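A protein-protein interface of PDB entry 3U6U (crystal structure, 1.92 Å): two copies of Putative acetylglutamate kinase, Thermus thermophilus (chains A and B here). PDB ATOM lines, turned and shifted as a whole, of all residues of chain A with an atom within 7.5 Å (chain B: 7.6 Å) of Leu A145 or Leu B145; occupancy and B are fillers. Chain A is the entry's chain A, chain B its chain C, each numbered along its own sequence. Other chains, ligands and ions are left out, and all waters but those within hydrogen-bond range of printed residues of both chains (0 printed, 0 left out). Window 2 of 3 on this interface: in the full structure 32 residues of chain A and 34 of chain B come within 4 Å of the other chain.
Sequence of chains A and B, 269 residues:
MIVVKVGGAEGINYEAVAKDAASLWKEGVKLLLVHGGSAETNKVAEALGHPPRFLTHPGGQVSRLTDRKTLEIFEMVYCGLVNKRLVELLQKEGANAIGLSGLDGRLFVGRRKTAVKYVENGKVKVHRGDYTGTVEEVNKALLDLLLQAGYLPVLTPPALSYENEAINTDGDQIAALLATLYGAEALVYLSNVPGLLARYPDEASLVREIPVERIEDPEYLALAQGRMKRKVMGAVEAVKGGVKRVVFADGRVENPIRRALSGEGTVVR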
ATOM      1  N   ASN A 139     -11.393   0.980  17.371  1.00  0.00           N
ATOM      2  CA  ASN A 139     -10.582   1.593  18.417  1.00  0.00           C
ATOM      3  C   ASN A 139     -11.424   1.518  19.689  1.00  0.00           C
ATOM      4  O   ASN A 139     -12.020   2.513  20.130  1.00  0.00           O
ATOM      5  CB  ASN A 139     -10.272   3.057  18.102  1.00  0.00           C
ATOM      6  CG  ASN A 139      -9.271   3.652  19.078  1.00  0.00           C
ATOM      7  OD1 ASN A 139      -9.097   3.142  20.185  1.00  0.00           O
ATOM      8  ND2 ASN A 139      -8.616   4.734  18.678  1.00  0.00           N
ATOM      9  N   LYS A 140     -11.480   0.330  20.274  1.00  0.00           N
ATOM     10  CA  LYS A 140     -12.266   0.123  21.479  1.00  0.00           C
ATOM     11  C   LYS A 140     -11.745   0.943  22.658  1.00  0.00           C
ATOM     12  O   LYS A 140     -12.516   1.340  23.532  1.00  0.00           O
ATOM     13  CB  LYS A 140     -12.286  -1.365  21.844  1.00  0.00           C
ATOM     14  CG  LYS A 140     -13.273  -1.710  22.954  1.00  0.00           C
ATOM     15  CD  LYS A 140     -13.424  -3.218  23.108  1.00  0.00           C
ATOM     16  CE  LYS A 140     -14.487  -3.566  24.143  1.00  0.00           C
ATOM     17  NZ  LYS A 140     -14.080  -3.162  25.520  1.00  0.00           N
ATOM     18  N   ALA A 141     -10.441   1.193  22.682  1.00  0.00           N
ATOM     19  CA  ALA A 141      -9.850   1.974  23.763  1.00  0.00           C
ATOM     20  C   ALA A 141     -10.445   3.381  23.771  1.00  0.00           C
ATOM     21  O   ALA A 141     -10.741   3.929  24.834  1.00  0.00           O
ATOM     22  CB  ALA A 141      -8.327   2.034  23.606  1.00  0.00           C
ATOM     23  N   LEU A 142     -10.621   3.963  22.588  1.00  0.00           N
ATOM     24  CA  LEU A 142     -11.199   5.302  22.487  1.00  0.00           C
ATOM     25  C   LEU A 142     -12.647   5.310  22.980  1.00  0.00           C
ATOM     26  O   LEU A 142     -13.051   6.210  23.717  1.00  0.00           O
ATOM     27  CB  LEU A 142     -11.151   5.800  21.041  1.00  0.00           C
ATOM     28  CG  LEU A 142     -11.907   7.106  20.755  1.00  0.00           C
ATOM     29  CD1 LEU A 142     -11.358   8.242  21.626  1.00  0.00           C
ATOM     30  CD2 LEU A 142     -11.760   7.450  19.279  1.00  0.00           C
ATOM     31  N   LEU A 143     -13.430   4.314  22.569  1.00  0.00           N
ATOM     32  CA  LEU A 143     -14.824   4.228  23.001  1.00  0.00           C
ATOM     33  C   LEU A 143     -14.908   4.020  24.512  1.00  0.00           C
ATOM     34  O   LEU A 143     -15.735   4.638  25.182  1.00  0.00           O
ATOM     35  CB  LEU A 143     -15.550   3.083  22.276  1.00  0.00           C
ATOM     36  CG  LEU A 143     -15.777   3.278  20.770  1.00  0.00           C
ATOM     37  CD1 LEU A 143     -16.535   2.079  20.190  1.00  0.00           C
ATOM     38  CD2 LEU A 143     -16.548   4.568  20.537  1.00  0.00           C
ATOM     39  N   ASP A 144     -14.053   3.154  25.047  1.00  0.00           N
ATOM     40  CA  ASP A 144     -14.056   2.889  26.484  1.00  0.00           C
ATOM     41  C   ASP A 144     -13.673   4.148  27.259  1.00  0.00           C
ATOM     42  O   ASP A 144     -14.219   4.427  28.326  1.00  0.00           O
ATOM     43  CB  ASP A 144     -13.095   1.742  26.831  1.00  0.00           C
ATOM     44  CG  ASP A 144     -13.620   0.379  26.381  1.00  0.00           C
ATOM     45  OD1 ASP A 144     -14.841   0.251  26.143  1.00  0.00           O
ATOM     46  OD2 ASP A 144     -12.812  -0.570  26.278  1.00  0.00           O
ATOM     47  N   LEU A 145     -12.734   4.907  26.709  1.00  0.00           N
ATOM     48  CA  LEU A 145     -12.294   6.151  27.327  1.00  0.00           C
ATOM     49  C   LEU A 145     -13.484   7.108  27.429  1.00  0.00           C
ATOM     50  O   LEU A 145     -13.732   7.696  28.483  1.00  0.00           O
ATOM     51  CB  LEU A 145     -11.192   6.791  26.477  1.00  0.00           C
ATOM     52  CG  LEU A 145     -10.563   8.088  26.981  1.00  0.00           C
ATOM     53  CD1 LEU A 145      -9.757   7.799  28.238  1.00  0.00           C
ATOM     54  CD2 LEU A 145      -9.661   8.680  25.897  1.00  0.00           C
ATOM     55  N   LEU A 146     -14.224   7.251  26.331  1.00  0.00           N
ATOM     56  CA  LEU A 146     -15.377   8.144  26.299  1.00  0.00           C
ATOM     57  C   LEU A 146     -16.527   7.633  27.164  1.00  0.00           C
ATOM     58  O   LEU A 146     -17.162   8.405  27.880  1.00  0.00           O
ATOM     59  CB  LEU A 146     -15.847   8.349  24.849  1.00  0.00           C
ATOM     60  CG  LEU A 146     -14.786   9.017  23.961  1.00  0.00           C
ATOM     61  CD1 LEU A 146     -15.192   8.954  22.495  1.00  0.00           C
ATOM     62  CD2 LEU A 146     -14.595  10.465  24.412  1.00  0.00           C
ATOM     63  N   LEU A 147     -16.796   6.332  27.101  1.00  0.00           N
ATOM     64  CA  LEU A 147     -17.864   5.758  27.914  1.00  0.00           C
ATOM     65  C   LEU A 147     -17.586   6.000  29.399  1.00  0.00           C
ATOM     66  O   LEU A 147     -18.473   6.396  30.154  1.00  0.00           O
ATOM     67  CB  LEU A 147     -17.980   4.252  27.654  1.00  0.00           C
ATOM     68  CG  LEU A 147     -18.539   3.844  26.287  1.00  0.00           C
ATOM     69  CD1 LEU A 147     -18.294   2.355  26.054  1.00  0.00           C
ATOM     70  CD2 LEU A 147     -20.027   4.170  26.229  1.00  0.00           C
ATOM     71  N   GLN A 148     -16.346   5.763  29.811  1.00  0.00           N
ATOM     72  CA  GLN A 148     -15.961   5.940  31.207  1.00  0.00           C
ATOM     73  C   GLN A 148     -16.011   7.406  31.653  1.00  0.00           C
ATOM     74  O   GLN A 148     -16.251   7.702  32.830  1.00  0.00           O
ATOM     75  CB  GLN A 148     -14.561   5.366  31.434  1.00  0.00           C
ATOM     76  CG  GLN A 148     -14.060   5.494  32.863  1.00  0.00           C
ATOM     77  CD  GLN A 148     -12.827   4.650  33.126  1.00  0.00           C
ATOM     78  OE1 GLN A 148     -12.865   3.423  33.012  1.00  0.00           O
ATOM     79  NE2 GLN A 148     -11.725   5.302  33.483  1.00  0.00           N
ATOM     80  N   ALA A 149     -15.799   8.319  30.708  1.00  0.00           N
ATOM     81  CA  ALA A 149     -15.824   9.745  31.010  1.00  0.00           C
ATOM     82  C   ALA A 149     -17.250  10.278  31.028  1.00  0.00           C
ATOM     83  O   ALA A 149     -17.471  11.459  31.271  1.00  0.00           O
ATOM     84  CB  ALA A 149     -14.979  10.517  29.990  1.00  0.00           C
ATOM     85  N   GLY A 150     -18.216   9.407  30.742  1.00  0.00           N
ATOM     86  CA  GLY A 150     -19.612   9.814  30.772  1.00  0.00           C
ATOM     87  C   GLY A 150     -20.252  10.306  29.483  1.00  0.00           C
ATOM     88  O   GLY A 150     -21.237  11.048  29.525  1.00  0.00           O
ATOM     89  N   TYR A 151     -19.716   9.902  28.339  1.00  0.00           N
ATOM     90  CA  TYR A 151     -20.273  10.325  27.055  1.00  0.00           C
ATOM     91  C   TYR A 151     -21.007   9.179  26.362  1.00  0.00           C
ATOM     92  O   TYR A 151     -20.687   8.013  26.579  1.00  0.00           O
ATOM     93  CB  TYR A 151     -19.155  10.839  26.142  1.00  0.00           C
ATOM     94  CG  TYR A 151     -18.439  12.044  26.705  1.00  0.00           C
ATOM     95  CD1 TYR A 151     -18.992  13.320  26.605  1.00  0.00           C
ATOM     96  CD2 TYR A 151     -17.236  11.900  27.388  1.00  0.00           C
ATOM     97  CE1 TYR A 151     -18.355  14.431  27.179  1.00  0.00           C
ATOM     98  CE2 TYR A 151     -16.594  12.997  27.969  1.00  0.00           C
ATOM     99  CZ  TYR A 151     -17.159  14.256  27.859  1.00  0.00           C
ATOM    100  OH  TYR A 151     -16.528  15.327  28.436  1.00  0.00           O
ATOM    101  N   TYR A 182     -18.006  -6.135  22.601  1.00  0.00           N
ATOM    102  CA  TYR A 182     -18.474  -5.794  23.942  1.00  0.00           C
ATOM    103  C   TYR A 182     -19.298  -6.894  24.603  1.00  0.00           C
ATOM    104  O   TYR A 182     -19.660  -6.781  25.771  1.00  0.00           O
ATOM    105  CB  TYR A 182     -19.314  -4.515  23.893  1.00  0.00           C
ATOM    106  CG  TYR A 182     -18.498  -3.244  23.855  1.00  0.00           C
ATOM    107  CD1 TYR A 182     -18.039  -2.655  25.032  1.00  0.00           C
ATOM    108  CD2 TYR A 182     -18.167  -2.642  22.641  1.00  0.00           C
ATOM    109  CE1 TYR A 182     -17.270  -1.497  25.005  1.00  0.00           C
ATOM    110  CE2 TYR A 182     -17.398  -1.481  22.603  1.00  0.00           C
ATOM    111  CZ  TYR A 182     -16.953  -0.917  23.789  1.00  0.00           C
ATOM    112  OH  TYR A 182     -16.190   0.226  23.759  1.00  0.00           O
ATOM    113  N   ASN B 139     -15.487  22.605  26.625  1.00  0.00           N
ATOM    114  CA  ASN B 139     -15.360  21.430  27.478  1.00  0.00           C
ATOM    115  C   ASN B 139     -13.866  21.086  27.452  1.00  0.00           C
ATOM    116  O   ASN B 139     -13.432  20.191  26.725  1.00  0.00           O
ATOM    117  CB  ASN B 139     -16.178  20.258  26.922  1.00  0.00           C
ATOM    118  CG  ASN B 139     -16.143  19.040  27.834  1.00  0.00           C
ATOM    119  OD1 ASN B 139     -15.287  18.939  28.715  1.00  0.00           O
ATOM    120  ND2 ASN B 139     -17.065  18.102  27.616  1.00  0.00           N
ATOM    121  N   LYS B 140     -13.075  21.812  28.239  1.00  0.00           N
ATOM    122  CA  LYS B 140     -11.639  21.584  28.258  1.00  0.00           C
ATOM    123  C   LYS B 140     -11.254  20.192  28.772  1.00  0.00           C
ATOM    124  O   LYS B 140     -10.252  19.630  28.346  1.00  0.00           O
ATOM    125  CB  LYS B 140     -10.934  22.665  29.092  1.00  0.00           C
ATOM    126  CG  LYS B 140      -9.405  22.620  28.973  1.00  0.00           C
ATOM    127  CD  LYS B 140      -8.762  23.867  29.552  1.00  0.00           C
ATOM    128  CE  LYS B 140      -7.246  23.848  29.382  1.00  0.00           C
ATOM    129  NZ  LYS B 140      -6.638  22.694  30.102  1.00  0.00           N
ATOM    130  N   ALA B 141     -12.046  19.640  29.685  1.00  0.00           N
ATOM    131  CA  ALA B 141     -11.748  18.312  30.215  1.00  0.00           C
ATOM    132  C   ALA B 141     -11.776  17.278  29.085  1.00  0.00           C
ATOM    133  O   ALA B 141     -10.947  16.371  29.045  1.00  0.00           O
ATOM    134  CB  ALA B 141     -12.752  17.936  31.315  1.00  0.00           C
ATOM    135  N   LEU B 142     -12.729  17.417  28.165  1.00  0.00           N
ATOM    136  CA  LEU B 142     -12.823  16.489  27.037  1.00  0.00           C
ATOM    137  C   LEU B 142     -11.600  16.619  26.136  1.00  0.00           C
ATOM    138  O   LEU B 142     -10.996  15.619  25.744  1.00  0.00           O
ATOM    139  CB  LEU B 142     -14.085  16.753  26.213  1.00  0.00           C
ATOM    140  CG  LEU B 142     -14.197  15.947  24.909  1.00  0.00           C
ATOM    141  CD1 LEU B 142     -14.167  14.436  25.203  1.00  0.00           C
ATOM    142  CD2 LEU B 142     -15.493  16.325  24.197  1.00  0.00           C
ATOM    143  N   LEU B 143     -11.231  17.854  25.803  1.00  0.00           N
ATOM    144  CA  LEU B 143     -10.065  18.067  24.957  1.00  0.00           C
ATOM    145  C   LEU B 143      -8.799  17.537  25.641  1.00  0.00           C
ATOM    146  O   LEU B 143      -7.969  16.894  25.004  1.00  0.00           O
ATOM    147  CB  LEU B 143      -9.907  19.561  24.627  1.00  0.00           C
ATOM    148  CG  LEU B 143     -10.960  20.149  23.677  1.00  0.00           C
ATOM    149  CD1 LEU B 143     -10.662  21.630  23.424  1.00  0.00           C
ATOM    150  CD2 LEU B 143     -10.956  19.379  22.359  1.00  0.00           C
ATOM    151  N   ASP B 144      -8.653  17.803  26.939  1.00  0.00           N
ATOM    152  CA  ASP B 144      -7.471  17.331  27.670  1.00  0.00           C
ATOM    153  C   ASP B 144      -7.424  15.801  27.679  1.00  0.00           C
ATOM    154  O   ASP B 144      -6.364  15.200  27.528  1.00  0.00           O
ATOM    155  CB  ASP B 144      -7.468  17.852  29.119  1.00  0.00           C
ATOM    156  CG  ASP B 144      -7.198  19.353  29.209  1.00  0.00           C
ATOM    157  OD1 ASP B 144      -6.594  19.921  28.273  1.00  0.00           O
ATOM    158  OD2 ASP B 144      -7.572  19.960  30.231  1.00  0.00           O
ATOM    159  N   LEU B 145      -8.582  15.181  27.856  1.00  0.00           N
ATOM    160  CA  LEU B 145      -8.674  13.727  27.866  1.00  0.00           C
ATOM    161  C   LEU B 145      -8.155  13.153  26.542  1.00  0.00           C
ATOM    162  O   LEU B 145      -7.377  12.200  26.523  1.00  0.00           O
ATOM    163  CB  LEU B 145     -10.131  13.308  28.061  1.00  0.00           C
ATOM    164  CG  LEU B 145     -10.421  11.814  28.191  1.00  0.00           C
ATOM    165  CD1 LEU B 145      -9.853  11.298  29.515  1.00  0.00           C
ATOM    166  CD2 LEU B 145     -11.926  11.587  28.132  1.00  0.00           C
ATOM    167  N   LEU B 146      -8.596  13.740  25.434  1.00  0.00           N
ATOM    168  CA  LEU B 146      -8.179  13.281  24.113  1.00  0.00           C
ATOM    169  C   LEU B 146      -6.706  13.583  23.836  1.00  0.00           C
ATOM    170  O   LEU B 146      -5.985  12.748  23.288  1.00  0.00           O
ATOM    171  CB  LEU B 146      -9.071  13.919  23.043  1.00  0.00           C
ATOM    172  CG  LEU B 146     -10.548  13.510  23.148  1.00  0.00           C
ATOM    173  CD1 LEU B 146     -11.400  14.320  22.164  1.00  0.00           C
ATOM    174  CD2 LEU B 146     -10.675  12.011  22.871  1.00  0.00           C
ATOM    175  N   LEU B 147      -6.260  14.776  24.209  1.00  0.00           N
ATOM    176  CA  LEU B 147      -4.861  15.152  24.002  1.00  0.00           C
ATOM    177  C   LEU B 147      -3.941  14.212  24.779  1.00  0.00           C
ATOM    178  O   LEU B 147      -2.940  13.729  24.253  1.00  0.00           O
ATOM    179  CB  LEU B 147      -4.623  16.597  24.456  1.00  0.00           C
ATOM    180  CG  LEU B 147      -5.243  17.685  23.567  1.00  0.00           C
ATOM    181  CD1 LEU B 147      -5.270  19.018  24.328  1.00  0.00           C
ATOM    182  CD2 LEU B 147      -4.443  17.804  22.263  1.00  0.00           C
ATOM    183  N   GLN B 148      -4.281  13.941  26.031  1.00  0.00           N
ATOM    184  CA  GLN B 148      -3.443  13.057  26.834  1.00  0.00           C
ATOM    185  C   GLN B 148      -3.472  11.624  26.329  1.00  0.00           C
ATOM    186  O   GLN B 148      -2.538  10.863  26.580  1.00  0.00           O
ATOM    187  CB  GLN B 148      -3.859  13.101  28.309  1.00  0.00           C
ATOM    188  CG  GLN B 148      -3.532  14.435  28.975  1.00  0.00           C
ATOM    189  CD  GLN B 148      -2.212  15.026  28.485  1.00  0.00           C
ATOM    190  OE1 GLN B 148      -1.130  14.511  28.783  1.00  0.00           O
ATOM    191  NE2 GLN B 148      -2.303  16.108  27.713  1.00  0.00           N
ATOM    192  N   ALA B 149      -4.535  11.257  25.616  1.00  0.00           N
ATOM    193  CA  ALA B 149      -4.650   9.902  25.083  1.00  0.00           C
ATOM    194  C   ALA B 149      -4.002   9.772  23.698  1.00  0.00           C
ATOM    195  O   ALA B 149      -4.068   8.714  23.078  1.00  0.00           O
ATOM    196  CB  ALA B 149      -6.115   9.482  25.019  1.00  0.00           C
ATOM    197  N   GLY B 150      -3.402  10.854  23.208  1.00  0.00           N
ATOM    198  CA  GLY B 150      -2.725  10.794  21.922  1.00  0.00           C
ATOM    199  C   GLY B 150      -3.518  11.139  20.669  1.00  0.00           C
ATOM    200  O   GLY B 150      -3.178  10.670  19.588  1.00  0.00           O
ATOM    201  N   TYR B 151      -4.563  11.952  20.798  1.00  0.00           N
ATOM    202  CA  TYR B 151      -5.362  12.338  19.633  1.00  0.00           C
ATOM    203  C   TYR B 151      -5.167  13.819  19.307  1.00  0.00           C
ATOM    204  O   TYR B 151      -4.935  14.632  20.207  1.00  0.00           O
ATOM    205  CB  TYR B 151      -6.843  12.056  19.902  1.00  0.00           C
ATOM    206  CG  TYR B 151      -7.120  10.589  20.152  1.00  0.00           C
ATOM    207  CD1 TYR B 151      -7.148   9.671  19.096  1.00  0.00           C
ATOM    208  CD2 TYR B 151      -7.284  10.102  21.451  1.00  0.00           C
ATOM    209  CE1 TYR B 151      -7.332   8.298  19.332  1.00  0.00           C
ATOM    210  CE2 TYR B 151      -7.466   8.739  21.695  1.00  0.00           C
ATOM    211  CZ  TYR B 151      -7.487   7.844  20.635  1.00  0.00           C
ATOM    212  OH  TYR B 151      -7.646   6.496  20.883  1.00  0.00           O
ATOM    213  N   TYR B 182      -5.702  27.688  27.142  1.00  0.00           N
ATOM    214  CA  TYR B 182      -4.490  26.871  27.175  1.00  0.00           C
ATOM    215  C   TYR B 182      -3.228  27.715  27.326  1.00  0.00           C
ATOM    216  O   TYR B 182      -2.131  27.172  27.425  1.00  0.00           O
ATOM    217  CB  TYR B 182      -4.378  26.040  25.887  1.00  0.00           C
ATOM    218  CG  TYR B 182      -5.200  24.772  25.909  1.00  0.00           C
ATOM    219  CD1 TYR B 182      -4.683  23.594  26.450  1.00  0.00           C
ATOM    220  CD2 TYR B 182      -6.509  24.760  25.430  1.00  0.00           C
ATOM    221  CE1 TYR B 182      -5.456  22.434  26.514  1.00  0.00           C
ATOM    222  CE2 TYR B 182      -7.289  23.609  25.494  1.00  0.00           C
ATOM    223  CZ  TYR B 182      -6.759  22.452  26.038  1.00  0.00           C
ATOM    224  OH  TYR B 182      -7.542  21.322  26.127  1.00  0.00           O
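Of the 14 printed residues of chain B, 5 touch a printed residue of chain A. Along chain B the printed residues that touch a printed residue of chain A span positions 139 to 151. Among the printed residues, no Asp or Glu carboxylate lies within 4 Å of a Lys or Arg side-chain nitrogen of the other chain.
N of Ala A141 lies close to OD1 of Asn A139, 3.4 Å away. OD1 of Asn A139 sits at hydrogen-bond distance from N of Leu A142 (3.0 Å). The backbone carbonyl oxygen (O) of Leu A146 is in hydrogen-bond range of the backbone NH (N) of Tyr A151 (3.0 Å). The backbone NH of Ala B141 lies close to the side-chain amide oxygen of Asn B139, at 3.5 Å. The side-chain amide oxygen (OD1) of Asn B139 is in hydrogen-bond range of the backbone NH (N) of Leu B142 (3.0 Å). O of Leu B146 lies within hydrogen-bond range of N of Tyr B151, at 3.0 Å.
Of the printed residues of chain B, Asn A139 touches Tyr B151. Of the printed residues of chain B, Leu A142 touches Tyr B151. Printed residues of chain B within 4 Å of Ala A149: Leu B145. Printed residues of chain A within 4 Å of Leu B145: Leu A145 (3.7 Å) and Ala A149 (3.7 Å). Of the printed residues of chain A, Tyr B151 touches Asn A139 (3.0 Å) and Leu A142 (3.6 Å). The nearest printed residue of chain A that does not touch Asn B139 is Ala A149 (7.6 Å).
Asn A139 touches Tyr B151, and with the chains exchanged Tyr A151 touches Asn B139. Leu A142 touches Tyr B151, and with the chains exchanged Tyr A151 touches Leu B142. Leu B145 touches its own counterpart, Leu A145. Leu A145 touches Ala B149, and with the chains exchanged Ala A149 touches Leu B145. Of the 7 pairs that touch across the chains among the printed residues, 7 have their exchanged pair printed and touching as well.
Among the printed residues, pairs that only touch across the chains: Leu A142 with Tyr B151, Leu A145 with Leu B145, Leu A145 with Ala B149, Ala A149 with Leu B145 and Tyr A151 with Leu B142.
The side-chain amide nitrogen of Asn A139 sits at hydrogen-bond distance from the side-chain hydroxyl of Tyr B151 (3.0 Å). The side-chain hydroxyl of Tyr A151 is in hydrogen-bond range of the side-chain amide nitrogen of Asn B139 (2.9 Å).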
